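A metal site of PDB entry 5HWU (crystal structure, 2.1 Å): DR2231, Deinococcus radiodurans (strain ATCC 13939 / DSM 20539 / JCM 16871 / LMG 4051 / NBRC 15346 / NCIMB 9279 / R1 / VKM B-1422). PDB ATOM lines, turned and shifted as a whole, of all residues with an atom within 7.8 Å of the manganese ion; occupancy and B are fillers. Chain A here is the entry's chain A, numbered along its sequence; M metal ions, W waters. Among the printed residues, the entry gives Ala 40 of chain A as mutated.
Within 4 Å of the manganese ion: Glu 41, Glu 44, Glu 73 and Asp 76.
OE1 of Glu 44 is bound to the manganese ion, at 2.1 Å.
The side-chain carboxylate (OD2) of Asp 76 is bound to the manganese ion (2.1 Å).
The side-chain carboxylate (OE1) of Glu 41 binds the manganese ion.
OE1 of Glu 73 binds the manganese ion, 2.3 Å away.
The manganese ion is bound by water W1, at 2.5 Å.
Water W2 is bound to the manganese ion.
The manganese ion has six donor atoms within binding distance.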
ATOM      1  N   LEU A  37     -19.603  -6.853 -12.852  1.00  0.00           N
ATOM      2  CA  LEU A  37     -18.852  -6.155 -11.814  1.00  0.00           C
ATOM      3  C   LEU A  37     -17.504  -6.823 -11.567  1.00  0.00           C
ATOM      4  O   LEU A  37     -16.473  -6.144 -11.473  1.00  0.00           O
ATOM      5  CB  LEU A  37     -19.678  -6.098 -10.524  1.00  0.00           C
ATOM      6  CG  LEU A  37     -21.067  -5.505 -10.729  1.00  0.00           C
ATOM      7  CD1 LEU A  37     -21.941  -5.529  -9.468  1.00  0.00           C
ATOM      8  CD2 LEU A  37     -20.944  -4.090 -11.300  1.00  0.00           C
ATOM      9  N   ALA A  40     -15.189  -5.925 -14.316  1.00  0.00           N
ATOM     10  CA  ALA A  40     -14.790  -4.525 -14.286  1.00  0.00           C
ATOM     11  C   ALA A  40     -13.670  -4.305 -13.286  1.00  0.00           C
ATOM     12  O   ALA A  40     -12.664  -3.653 -13.589  1.00  0.00           O
ATOM     13  CB  ALA A  40     -15.995  -3.643 -13.966  1.00  0.00           C
ATOM     14  N   GLU A  41     -13.809  -4.845 -12.075  1.00  0.00           N
ATOM     15  CA  GLU A  41     -12.752  -4.656 -11.088  1.00  0.00           C
ATOM     16  C   GLU A  41     -11.538  -5.525 -11.383  1.00  0.00           C
ATOM     17  O   GLU A  41     -10.412  -5.133 -11.070  1.00  0.00           O
ATOM     18  CB  GLU A  41     -13.275  -4.908  -9.671  1.00  0.00           C
ATOM     19  CG  GLU A  41     -14.465  -4.034  -9.256  1.00  0.00           C
ATOM     20  CD  GLU A  41     -14.189  -2.525  -9.319  1.00  0.00           C
ATOM     21  OE1 GLU A  41     -13.010  -2.117  -9.251  1.00  0.00           O
ATOM     22  OE2 GLU A  41     -15.154  -1.748  -9.458  1.00  0.00           O
ATOM     23  N   SER A  42     -11.736  -6.702 -12.004  1.00  0.00           N
ATOM     24  CA  SER A  42     -10.597  -7.509 -12.417  1.00  0.00           C
ATOM     25  C   SER A  42      -9.728  -6.755 -13.403  1.00  0.00           C
ATOM     26  O   SER A  42      -8.495  -6.793 -13.313  1.00  0.00           O
ATOM     27  CB  SER A  42     -11.049  -8.827 -13.054  1.00  0.00           C
ATOM     28  OG  SER A  42     -11.907  -9.512 -12.180  1.00  0.00           O
ATOM     29  N   GLU A  44      -9.499  -3.477 -13.774  1.00  0.00           N
ATOM     30  CA  GLU A  44      -8.828  -2.368 -13.111  1.00  0.00           C
ATOM     31  C   GLU A  44      -7.633  -2.852 -12.288  1.00  0.00           C
ATOM     32  O   GLU A  44      -6.611  -2.171 -12.204  1.00  0.00           O
ATOM     33  CB  GLU A  44      -9.814  -1.608 -12.229  1.00  0.00           C
ATOM     34  CG  GLU A  44     -10.840  -0.781 -13.014  1.00  0.00           C
ATOM     35  CD  GLU A  44     -12.102  -0.506 -12.224  1.00  0.00           C
ATOM     36  OE1 GLU A  44     -12.030   0.181 -11.192  1.00  0.00           O
ATOM     37  OE2 GLU A  44     -13.168  -1.041 -12.614  1.00  0.00           O
ATOM     38  N   VAL A  45      -7.743  -4.038 -11.685  1.00  0.00           N
ATOM     39  CA  VAL A  45      -6.600  -4.611 -10.974  1.00  0.00           C
ATOM     40  C   VAL A  45      -5.487  -4.951 -11.949  1.00  0.00           C
ATOM     41  O   VAL A  45      -4.311  -4.617 -11.721  1.00  0.00           O
ATOM     42  CB  VAL A  45      -7.017  -5.852 -10.162  1.00  0.00           C
ATOM     43  CG1 VAL A  45      -5.791  -6.530  -9.575  1.00  0.00           C
ATOM     44  CG2 VAL A  45      -7.993  -5.466  -9.043  1.00  0.00           C
ATOM     45  N   PRO A  69      -2.975   2.892  -5.802  1.00  0.00           N
ATOM     46  CA  PRO A  69      -3.982   2.548  -6.824  1.00  0.00           C
ATOM     47  C   PRO A  69      -4.255   1.054  -6.956  1.00  0.00           C
ATOM     48  O   PRO A  69      -5.404   0.647  -7.178  1.00  0.00           O
ATOM     49  CB  PRO A  69      -3.381   3.125  -8.115  1.00  0.00           C
ATOM     50  CG  PRO A  69      -2.451   4.207  -7.652  1.00  0.00           C
ATOM     51  CD  PRO A  69      -1.867   3.687  -6.375  1.00  0.00           C
ATOM     52  N   HIS A  72      -6.208  -0.077  -3.875  1.00  0.00           N
ATOM     53  CA  HIS A  72      -7.584   0.367  -4.010  1.00  0.00           C
ATOM     54  C   HIS A  72      -8.378  -0.605  -4.872  1.00  0.00           C
ATOM     55  O   HIS A  72      -9.461  -1.067  -4.491  1.00  0.00           O
ATOM     56  CB  HIS A  72      -7.595   1.776  -4.612  1.00  0.00           C
ATOM     57  CG  HIS A  72      -8.938   2.436  -4.595  1.00  0.00           C
ATOM     58  ND1 HIS A  72      -9.101   3.787  -4.340  1.00  0.00           N
ATOM     59  CD2 HIS A  72     -10.190   1.941  -4.812  1.00  0.00           C
ATOM     60  CE1 HIS A  72     -10.393   4.091  -4.395  1.00  0.00           C
ATOM     61  NE2 HIS A  72     -11.071   2.987  -4.678  1.00  0.00           N
ATOM     62  N   GLU A  73      -7.840  -0.943  -6.048  1.00  0.00           N
ATOM     63  CA  GLU A  73      -8.557  -1.824  -6.977  1.00  0.00           C
ATOM     64  C   GLU A  73      -8.702  -3.225  -6.422  1.00  0.00           C
ATOM     65  O   GLU A  73      -9.697  -3.903  -6.722  1.00  0.00           O
ATOM     66  CB  GLU A  73      -7.855  -1.850  -8.334  1.00  0.00           C
ATOM     67  CG  GLU A  73      -7.859  -0.508  -9.044  1.00  0.00           C
ATOM     68  CD  GLU A  73      -9.262   0.068  -9.186  1.00  0.00           C
ATOM     69  OE1 GLU A  73     -10.226  -0.733  -9.237  1.00  0.00           O
ATOM     70  OE2 GLU A  73      -9.411   1.296  -9.267  1.00  0.00           O
ATOM     71  N   LEU A  74      -7.757  -3.674  -5.599  1.00  0.00           N
ATOM     72  CA  LEU A  74      -7.899  -4.985  -4.957  1.00  0.00           C
ATOM     73  C   LEU A  74      -9.025  -4.973  -3.928  1.00  0.00           C
ATOM     74  O   LEU A  74      -9.790  -5.947  -3.834  1.00  0.00           O
ATOM     75  CB  LEU A  74      -6.580  -5.391  -4.326  1.00  0.00           C
ATOM     76  CG  LEU A  74      -5.468  -5.681  -5.325  1.00  0.00           C
ATOM     77  CD1 LEU A  74      -4.111  -5.677  -4.616  1.00  0.00           C
ATOM     78  CD2 LEU A  74      -5.732  -7.024  -5.993  1.00  0.00           C
ATOM     79  N   ALA A  75      -9.133  -3.896  -3.148  1.00  0.00           N
ATOM     80  CA  ALA A  75     -10.280  -3.747  -2.252  1.00  0.00           C
ATOM     81  C   ALA A  75     -11.587  -3.664  -3.045  1.00  0.00           C
ATOM     82  O   ALA A  75     -12.599  -4.249  -2.634  1.00  0.00           O
ATOM     83  CB  ALA A  75     -10.099  -2.499  -1.393  1.00  0.00           C
ATOM     84  N   ASP A  76     -11.579  -2.951  -4.167  1.00  0.00           N
ATOM     85  CA  ASP A  76     -12.745  -2.919  -5.052  1.00  0.00           C
ATOM     86  C   ASP A  76     -13.124  -4.320  -5.509  1.00  0.00           C
ATOM     87  O   ASP A  76     -14.321  -4.636  -5.632  1.00  0.00           O
ATOM     88  CB  ASP A  76     -12.454  -2.042  -6.268  1.00  0.00           C
ATOM     89  CG  ASP A  76     -12.796  -0.575  -6.052  1.00  0.00           C
ATOM     90  OD1 ASP A  76     -13.199  -0.222  -4.925  1.00  0.00           O
ATOM     91  OD2 ASP A  76     -12.652   0.219  -7.002  1.00  0.00           O
ATOM     92  N   LEU A  77     -12.134  -5.165  -5.801  1.00  0.00           N
ATOM     93  CA  LEU A  77     -12.447  -6.518  -6.245  1.00  0.00           C
ATOM     94  C   LEU A  77     -12.951  -7.378  -5.082  1.00  0.00           C
ATOM     95  O   LEU A  77     -13.900  -8.146  -5.248  1.00  0.00           O
ATOM     96  CB  LEU A  77     -11.218  -7.132  -6.913  1.00  0.00           C
ATOM     97  CG  LEU A  77     -11.313  -8.514  -7.571  1.00  0.00           C
ATOM     98  CD1 LEU A  77     -12.391  -8.563  -8.624  1.00  0.00           C
ATOM     99  CD2 LEU A  77      -9.960  -8.882  -8.190  1.00  0.00           C
ATOM    100  N   VAL A  80     -16.802  -6.348  -4.693  1.00  0.00           N
ATOM    101  CA  VAL A  80     -17.788  -6.937  -5.593  1.00  0.00           C
ATOM    102  C   VAL A  80     -17.809  -8.462  -5.500  1.00  0.00           C
ATOM    103  O   VAL A  80     -18.780  -9.072  -5.951  1.00  0.00           O
ATOM    104  CB  VAL A  80     -17.573  -6.518  -7.058  1.00  0.00           C
ATOM    105  CG1 VAL A  80     -17.529  -5.011  -7.165  1.00  0.00           C
ATOM    106  CG2 VAL A  80     -16.301  -7.148  -7.635  1.00  0.00           C
HETATM  107 MN    MN M   1     -12.376   0.034  -9.117  1.00  0.00          MN
HETATM  108  O   HOH W   1     -14.711   0.863  -9.493  1.00  0.00           O
HETATM  109  O   HOH W   2     -11.865   2.544  -8.937  1.00  0.00           O
